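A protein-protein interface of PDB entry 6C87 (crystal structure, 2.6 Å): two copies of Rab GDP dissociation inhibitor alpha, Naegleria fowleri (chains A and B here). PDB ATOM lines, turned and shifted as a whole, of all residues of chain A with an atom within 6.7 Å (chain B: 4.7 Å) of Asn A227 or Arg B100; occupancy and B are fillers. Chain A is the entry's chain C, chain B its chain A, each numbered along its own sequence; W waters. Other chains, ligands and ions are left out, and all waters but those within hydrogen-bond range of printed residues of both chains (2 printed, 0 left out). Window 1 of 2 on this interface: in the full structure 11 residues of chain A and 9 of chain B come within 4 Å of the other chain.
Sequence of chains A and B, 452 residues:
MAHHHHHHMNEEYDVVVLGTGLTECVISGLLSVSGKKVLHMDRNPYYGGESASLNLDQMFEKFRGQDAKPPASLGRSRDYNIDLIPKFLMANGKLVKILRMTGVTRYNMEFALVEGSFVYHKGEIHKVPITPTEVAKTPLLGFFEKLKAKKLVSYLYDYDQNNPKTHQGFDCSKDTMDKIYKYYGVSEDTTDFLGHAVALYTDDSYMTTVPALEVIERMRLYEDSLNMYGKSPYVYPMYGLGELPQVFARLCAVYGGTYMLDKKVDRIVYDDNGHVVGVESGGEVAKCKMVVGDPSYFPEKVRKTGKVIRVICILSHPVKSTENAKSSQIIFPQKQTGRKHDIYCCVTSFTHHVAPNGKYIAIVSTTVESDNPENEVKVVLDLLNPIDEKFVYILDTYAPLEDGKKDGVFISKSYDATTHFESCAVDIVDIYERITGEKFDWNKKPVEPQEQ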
ATOM      1  N   TYR A 222      34.899 -24.597   7.064  1.00  0.00           N
ATOM      2  CA  TYR A 222      34.277 -25.617   7.897  1.00  0.00           C
ATOM      3  C   TYR A 222      33.240 -24.990   8.815  1.00  0.00           C
ATOM      4  O   TYR A 222      32.089 -25.438   8.882  1.00  0.00           O
ATOM      5  CB  TYR A 222      35.345 -26.336   8.721  1.00  0.00           C
ATOM      6  CG  TYR A 222      34.880 -27.609   9.410  1.00  0.00           C
ATOM      7  CD1 TYR A 222      35.399 -28.848   9.034  1.00  0.00           C
ATOM      8  CD2 TYR A 222      33.959 -27.578  10.453  1.00  0.00           C
ATOM      9  CE1 TYR A 222      35.004 -30.019   9.663  1.00  0.00           C
ATOM     10  CE2 TYR A 222      33.542 -28.747  11.075  1.00  0.00           C
ATOM     11  CZ  TYR A 222      34.079 -29.960  10.682  1.00  0.00           C
ATOM     12  OH  TYR A 222      33.686 -31.121  11.301  1.00  0.00           O
ATOM     13  N   GLU A 223      33.629 -23.926   9.516  1.00  0.00           N
ATOM     14  CA  GLU A 223      32.701 -23.292  10.437  1.00  0.00           C
ATOM     15  C   GLU A 223      31.523 -22.682   9.693  1.00  0.00           C
ATOM     16  O   GLU A 223      30.378 -22.790  10.147  1.00  0.00           O
ATOM     17  CB  GLU A 223      33.424 -22.236  11.262  1.00  0.00           C
ATOM     18  CG  GLU A 223      33.034 -22.268  12.719  1.00  0.00           C
ATOM     19  CD  GLU A 223      33.023 -20.896  13.345  1.00  0.00           C
ATOM     20  OE1 GLU A 223      33.923 -20.089  13.029  1.00  0.00           O
ATOM     21  OE2 GLU A 223      32.102 -20.619  14.141  1.00  0.00           O
ATOM     22  N   ASP A 224      31.776 -22.067   8.533  1.00  0.00           N
ATOM     23  CA  ASP A 224      30.687 -21.481   7.755  1.00  0.00           C
ATOM     24  C   ASP A 224      29.707 -22.552   7.299  1.00  0.00           C
ATOM     25  O   ASP A 224      28.486 -22.373   7.395  1.00  0.00           O
ATOM     26  CB  ASP A 224      31.226 -20.716   6.549  1.00  0.00           C
ATOM     27  CG  ASP A 224      31.711 -19.331   6.905  1.00  0.00           C
ATOM     28  OD1 ASP A 224      31.265 -18.794   7.943  1.00  0.00           O
ATOM     29  OD2 ASP A 224      32.503 -18.762   6.122  1.00  0.00           O
ATOM     30  N   SER A 225      30.229 -23.668   6.776  1.00  0.00           N
ATOM     31  CA  SER A 225      29.362 -24.751   6.323  1.00  0.00           C
ATOM     32  C   SER A 225      28.560 -25.331   7.484  1.00  0.00           C
ATOM     33  O   SER A 225      27.375 -25.658   7.334  1.00  0.00           O
ATOM     34  CB  SER A 225      30.199 -25.843   5.647  1.00  0.00           C
ATOM     35  OG  SER A 225      30.859 -25.376   4.483  1.00  0.00           O
ATOM     36  N   LEU A 226      29.194 -25.470   8.648  1.00  0.00           N
ATOM     37  CA  LEU A 226      28.507 -25.992   9.822  1.00  0.00           C
ATOM     38  C   LEU A 226      27.389 -25.058  10.282  1.00  0.00           C
ATOM     39  O   LEU A 226      26.338 -25.513  10.750  1.00  0.00           O
ATOM     40  CB  LEU A 226      29.526 -26.229  10.932  1.00  0.00           C
ATOM     41  CG  LEU A 226      29.021 -26.507  12.340  1.00  0.00           C
ATOM     42  CD1 LEU A 226      28.404 -27.883  12.413  1.00  0.00           C
ATOM     43  CD2 LEU A 226      30.183 -26.382  13.295  1.00  0.00           C
ATOM     44  N   ASN A 227      27.610 -23.747  10.182  1.00  0.00           N
ATOM     45  CA  ASN A 227      26.624 -22.750  10.589  1.00  0.00           C
ATOM     46  C   ASN A 227      25.421 -22.668   9.658  1.00  0.00           C
ATOM     47  O   ASN A 227      24.459 -21.968   9.996  1.00  0.00           O
ATOM     48  CB  ASN A 227      27.253 -21.356  10.693  1.00  0.00           C
ATOM     49  CG  ASN A 227      28.053 -21.162  11.969  1.00  0.00           C
ATOM     50  OD1 ASN A 227      27.851 -21.866  12.960  1.00  0.00           O
ATOM     51  ND2 ASN A 227      28.950 -20.177  11.958  1.00  0.00           N
ATOM     52  N   MET A 228      25.458 -23.302   8.483  1.00  0.00           N
ATOM     53  CA  MET A 228      24.368 -23.105   7.530  1.00  0.00           C
ATOM     54  C   MET A 228      23.103 -23.850   7.948  1.00  0.00           C
ATOM     55  O   MET A 228      22.005 -23.278   7.934  1.00  0.00           O
ATOM     56  CB  MET A 228      24.796 -23.562   6.138  1.00  0.00           C
ATOM     57  CG  MET A 228      25.486 -22.490   5.344  1.00  0.00           C
ATOM     58  SD  MET A 228      25.690 -22.949   3.623  1.00  0.00           S
ATOM     59  CE  MET A 228      23.999 -22.890   3.042  1.00  0.00           C
ATOM     60  N   TYR A 229      23.227 -25.138   8.283  1.00  0.00           N
ATOM     61  CA  TYR A 229      22.085 -25.932   8.712  1.00  0.00           C
ATOM     62  C   TYR A 229      22.268 -26.548  10.087  1.00  0.00           C
ATOM     63  O   TYR A 229      21.270 -26.836  10.754  1.00  0.00           O
ATOM     64  CB  TYR A 229      21.822 -27.071   7.714  1.00  0.00           C
ATOM     65  CG  TYR A 229      21.817 -26.615   6.277  1.00  0.00           C
ATOM     66  CD1 TYR A 229      20.844 -25.748   5.790  1.00  0.00           C
ATOM     67  CD2 TYR A 229      22.811 -27.036   5.412  1.00  0.00           C
ATOM     68  CE1 TYR A 229      20.868 -25.327   4.475  1.00  0.00           C
ATOM     69  CE2 TYR A 229      22.843 -26.623   4.110  1.00  0.00           C
ATOM     70  CZ  TYR A 229      21.875 -25.773   3.640  1.00  0.00           C
ATOM     71  OH  TYR A 229      21.931 -25.373   2.326  1.00  0.00           O
ATOM     72  N   GLY A 230      23.505 -26.716  10.540  1.00  0.00           N
ATOM     73  CA  GLY A 230      23.820 -27.288  11.830  1.00  0.00           C
ATOM     74  C   GLY A 230      24.311 -28.722  11.705  1.00  0.00           C
ATOM     75  O   GLY A 230      24.322 -29.324  10.628  1.00  0.00           O
ATOM     76  N   SER A 232      26.843 -30.619  11.176  1.00  0.00           N
ATOM     77  CA  SER A 232      28.119 -30.919  10.534  1.00  0.00           C
ATOM     78  C   SER A 232      28.256 -30.009   9.324  1.00  0.00           C
ATOM     79  O   SER A 232      27.278 -29.379   8.898  1.00  0.00           O
ATOM     80  CB  SER A 232      28.229 -32.403  10.128  1.00  0.00           C
ATOM     81  OG  SER A 232      27.791 -32.629   8.804  1.00  0.00           O
ATOM     82  N   PRO A 233      29.451 -29.912   8.742  1.00  0.00           N
ATOM     83  CA  PRO A 233      29.614 -29.066   7.554  1.00  0.00           C
ATOM     84  C   PRO A 233      29.227 -29.754   6.259  1.00  0.00           C
ATOM     85  O   PRO A 233      29.345 -29.145   5.191  1.00  0.00           O
ATOM     86  CB  PRO A 233      31.119 -28.745   7.574  1.00  0.00           C
ATOM     87  CG  PRO A 233      31.728 -29.981   8.152  1.00  0.00           C
ATOM     88  CD  PRO A 233      30.743 -30.458   9.207  1.00  0.00           C
ATOM     89  N   ALA B  91      18.238 -15.742   6.980  1.00  0.00           N
ATOM     90  CA  ALA B  91      19.287 -16.758   7.060  1.00  0.00           C
ATOM     91  C   ALA B  91      20.575 -16.285   7.731  1.00  0.00           C
ATOM     92  O   ALA B  91      21.226 -17.066   8.435  1.00  0.00           O
ATOM     93  CB  ALA B  91      19.594 -17.286   5.663  1.00  0.00           C
ATOM     94  N   ASN B  92      20.973 -15.029   7.536  1.00  0.00           N
ATOM     95  CA  ASN B  92      22.184 -14.574   8.227  1.00  0.00           C
ATOM     96  C   ASN B  92      21.932 -13.284   8.997  1.00  0.00           C
ATOM     97  O   ASN B  92      22.823 -12.436   9.111  1.00  0.00           O
ATOM     98  CB  ASN B  92      23.351 -14.402   7.252  1.00  0.00           C
ATOM     99  CG  ASN B  92      24.146 -15.686   7.052  1.00  0.00           C
ATOM    100  OD1 ASN B  92      24.577 -16.320   8.016  1.00  0.00           O
ATOM    101  ND2 ASN B  92      24.334 -16.078   5.798  1.00  0.00           N
ATOM    102  N   VAL B  96      19.939 -15.142  14.011  1.00  0.00           N
ATOM    103  CA  VAL B  96      20.835 -16.255  13.712  1.00  0.00           C
ATOM    104  C   VAL B  96      22.217 -15.999  14.308  1.00  0.00           C
ATOM    105  O   VAL B  96      22.873 -16.918  14.817  1.00  0.00           O
ATOM    106  CB  VAL B  96      20.900 -16.487  12.190  1.00  0.00           C
ATOM    107  CG1 VAL B  96      22.057 -17.402  11.833  1.00  0.00           C
ATOM    108  CG2 VAL B  96      19.585 -17.067  11.686  1.00  0.00           C
ATOM    109  N   LYS B  97      22.689 -14.749  14.244  1.00  0.00           N
ATOM    110  CA  LYS B  97      24.000 -14.436  14.804  1.00  0.00           C
ATOM    111  C   LYS B  97      23.991 -14.498  16.328  1.00  0.00           C
ATOM    112  O   LYS B  97      24.944 -14.997  16.938  1.00  0.00           O
ATOM    113  CB  LYS B  97      24.475 -13.066  14.312  1.00  0.00           C
ATOM    114  CG  LYS B  97      24.935 -13.088  12.858  1.00  0.00           C
ATOM    115  CD  LYS B  97      25.448 -11.743  12.373  1.00  0.00           C
ATOM    116  CE  LYS B  97      25.903 -11.846  10.925  1.00  0.00           C
ATOM    117  NZ  LYS B  97      26.623 -10.630  10.467  1.00  0.00           N
ATOM    118  N   ILE B  98      22.913 -14.026  16.962  1.00  0.00           N
ATOM    119  CA  ILE B  98      22.825 -14.106  18.416  1.00  0.00           C
ATOM    120  C   ILE B  98      22.751 -15.560  18.868  1.00  0.00           C
ATOM    121  O   ILE B  98      23.408 -15.955  19.838  1.00  0.00           O
ATOM    122  CB  ILE B  98      21.614 -13.311  18.924  1.00  0.00           C
ATOM    123  CG1 ILE B  98      21.683 -11.859  18.464  1.00  0.00           C
ATOM    124  CG2 ILE B  98      21.573 -13.343  20.438  1.00  0.00           C
ATOM    125  CD1 ILE B  98      20.431 -11.061  18.822  1.00  0.00           C
ATOM    126  N   LEU B  99      21.946 -16.372  18.173  1.00  0.00           N
ATOM    127  CA  LEU B  99      21.850 -17.795  18.485  1.00  0.00           C
ATOM    128  C   LEU B  99      23.204 -18.481  18.363  1.00  0.00           C
ATOM    129  O   LEU B  99      23.535 -19.363  19.165  1.00  0.00           O
ATOM    130  CB  LEU B  99      20.842 -18.455  17.549  1.00  0.00           C
ATOM    131  CG  LEU B  99      19.382 -18.074  17.769  1.00  0.00           C
ATOM    132  CD1 LEU B  99      18.478 -18.771  16.752  1.00  0.00           C
ATOM    133  CD2 LEU B  99      18.985 -18.413  19.206  1.00  0.00           C
ATOM    134  N   ARG B 100      24.001 -18.090  17.365  1.00  0.00           N
ATOM    135  CA  ARG B 100      25.336 -18.657  17.224  1.00  0.00           C
ATOM    136  C   ARG B 100      26.227 -18.286  18.400  1.00  0.00           C
ATOM    137  O   ARG B 100      27.043 -19.100  18.846  1.00  0.00           O
ATOM    138  CB  ARG B 100      25.974 -18.213  15.909  1.00  0.00           C
ATOM    139  CG  ARG B 100      25.533 -19.018  14.694  1.00  0.00           C
ATOM    140  CD  ARG B 100      25.977 -18.370  13.386  1.00  0.00           C
ATOM    141  NE  ARG B 100      25.251 -18.928  12.252  1.00  0.00           N
ATOM    142  CZ  ARG B 100      25.235 -18.403  11.028  1.00  0.00           C
ATOM    143  NH1 ARG B 100      25.903 -17.283  10.774  1.00  0.00           N
ATOM    144  NH2 ARG B 100      24.538 -18.994  10.060  1.00  0.00           N
ATOM    145  N   MET B 101      26.080 -17.067  18.922  1.00  0.00           N
ATOM    146  CA  MET B 101      26.900 -16.631  20.046  1.00  0.00           C
ATOM    147  C   MET B 101      26.676 -17.496  21.281  1.00  0.00           C
ATOM    148  O   MET B 101      27.616 -17.758  22.043  1.00  0.00           O
ATOM    149  CB  MET B 101      26.594 -15.175  20.367  1.00  0.00           C
ATOM    150  CG  MET B 101      27.150 -14.180  19.388  1.00  0.00           C
ATOM    151  SD  MET B 101      26.557 -12.554  19.869  1.00  0.00           S
ATOM    152  CE  MET B 101      27.790 -12.139  21.103  1.00  0.00           C
ATOM    153  N   THR B 102      25.439 -17.947  21.500  1.00  0.00           N
ATOM    154  CA  THR B 102      25.168 -18.807  22.648  1.00  0.00           C
ATOM    155  C   THR B 102      25.668 -20.228  22.434  1.00  0.00           C
ATOM    156  O   THR B 102      25.913 -20.942  23.410  1.00  0.00           O
ATOM    157  CB  THR B 102      23.669 -18.880  22.931  1.00  0.00           C
ATOM    158  OG1 THR B 102      23.022 -19.542  21.837  1.00  0.00           O
ATOM    159  CG2 THR B 102      23.069 -17.480  23.115  1.00  0.00           C
ATOM    160  N   GLY B 103      25.801 -20.668  21.186  1.00  0.00           N
ATOM    161  CA  GLY B 103      26.213 -22.025  20.921  1.00  0.00           C
ATOM    162  C   GLY B 103      25.083 -23.030  20.847  1.00  0.00           C
ATOM    163  O   GLY B 103      25.350 -24.214  20.602  1.00  0.00           O
ATOM    164  N   THR B 105      22.979 -23.407  18.585  1.00  0.00           N
ATOM    165  CA  THR B 105      22.796 -23.859  17.208  1.00  0.00           C
ATOM    166  C   THR B 105      23.651 -25.073  16.867  1.00  0.00           C
ATOM    167  O   THR B 105      23.337 -25.779  15.901  1.00  0.00           O
ATOM    168  CB  THR B 105      23.096 -22.721  16.219  1.00  0.00           C
ATOM    169  OG1 THR B 105      24.360 -22.117  16.527  1.00  0.00           O
ATOM    170  CG2 THR B 105      22.000 -21.669  16.245  1.00  0.00           C
ATOM    171  N   ARG B 106      24.716 -25.329  17.633  1.00  0.00           N
ATOM    172  CA  ARG B 106      25.581 -26.483  17.414  1.00  0.00           C
ATOM    173  C   ARG B 106      25.029 -27.770  18.017  1.00  0.00           C
ATOM    174  O   ARG B 106      25.606 -28.840  17.790  1.00  0.00           O
ATOM    175  CB  ARG B 106      26.978 -26.205  17.983  1.00  0.00           C
ATOM    176  CG  ARG B 106      27.986 -25.755  16.942  1.00  0.00           C
ATOM    177  CD  ARG B 106      29.153 -25.002  17.555  1.00  0.00           C
ATOM    178  NE  ARG B 106      30.092 -24.549  16.530  1.00  0.00           N
ATOM    179  CZ  ARG B 106      29.946 -23.436  15.814  1.00  0.00           C
ATOM    180  NH1 ARG B 106      28.894 -22.652  16.006  1.00  0.00           N
ATOM    181  NH2 ARG B 106      30.853 -23.109  14.903  1.00  0.00           N
ATOM    182  N   TYR B 229      20.533 -20.505   0.166  1.00  0.00           N
ATOM    183  CA  TYR B 229      19.542 -21.529   0.450  1.00  0.00           C
ATOM    184  C   TYR B 229      18.609 -21.795  -0.720  1.00  0.00           C
ATOM    185  O   TYR B 229      17.913 -22.814  -0.716  1.00  0.00           O
ATOM    186  CB  TYR B 229      18.759 -21.157   1.725  1.00  0.00           C
ATOM    187  CG  TYR B 229      19.702 -20.994   2.904  1.00  0.00           C
ATOM    188  CD1 TYR B 229      19.926 -22.049   3.777  1.00  0.00           C
ATOM    189  CD2 TYR B 229      20.426 -19.819   3.100  1.00  0.00           C
ATOM    190  CE1 TYR B 229      20.815 -21.931   4.835  1.00  0.00           C
ATOM    191  CE2 TYR B 229      21.322 -19.696   4.150  1.00  0.00           C
ATOM    192  CZ  TYR B 229      21.508 -20.755   5.020  1.00  0.00           C
ATOM    193  OH  TYR B 229      22.395 -20.643   6.074  1.00  0.00           O
HETATM  194  O   HOH W   1      23.495 -21.250  12.661  1.00  0.00           O
HETATM  195  O   HOH W   2      28.652 -18.338   9.199  1.00  0.00           O
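Water W1 bridges the backbone carbonyl oxygen (O) of Asn A227 (2.9 Å) and the guanidinium group (NE) of Arg B100 (2.9 Å).
Water W2 lies within hydrogen-bond range of OD1 of Asp A224 (2.9 Å), ND2 of Asn A227 (3.3 Å) and NH1 of Arg B100 (3.3 Å).
Leu A226 touches Arg B106.
CE1 of Tyr A229 touches CE1 of Tyr B229, at 3.4 Å.
Of the 11 printed residues of chain A, 5 touch a printed residue of chain B.
Printed residues of chain B that touch a printed residue of chain A: Arg B100, Arg B106 and Tyr B229.
Hydrophobic or aromatic side chains of chain B within 4 Å of the printed part of chain A: Tyr B229.
Among the printed residues, Asp or Glu carboxylates within 4 Å of a Lys or Arg side-chain nitrogen of the other chain: Glu A223 with Arg B106.
The guanidinium group of Arg B100 lies within hydrogen-bond range of the backbone carbonyl oxygen of Asn A227, at 3.0 Å.
The guanidinium group of Arg B106 is in salt-bridge range of the side-chain carboxylate of Glu A223 (2.9 Å).
The guanidinium group (NH1) of Arg B106 lies within hydrogen-bond range of the side-chain amide oxygen (OD1) of Asn A227, at 3.3 Å.
The side-chain hydroxyl (OH) of Tyr B229 is in hydrogen-bond range of the backbone carbonyl oxygen (O) of Met A228 (3.2 Å).
Of the printed residues of chain B, Leu A226 touches Arg B106.
Asn A227 touches just these residues of chain B: Arg B100 and Arg B106.
Of the printed residues of chain B, Tyr A229 touches Tyr B229.
Printed residues of chain A within 4 Å of Arg B106: Glu A223 (2.9 Å), Leu A226 (3.7 Å) and Asn A227 (3.3 Å).
The nearest residue of chain A that does not touch Arg B100 is Met A228 (4.7 Å).
Tyr B229 touches its own counterpart, Tyr A229.
OD1 of Asn B92 is in hydrogen-bond range of NH1 of Arg B100, at 3.2 Å.
O of Glu A223 sits close to ND2 of Asn A227 (3.5 Å).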
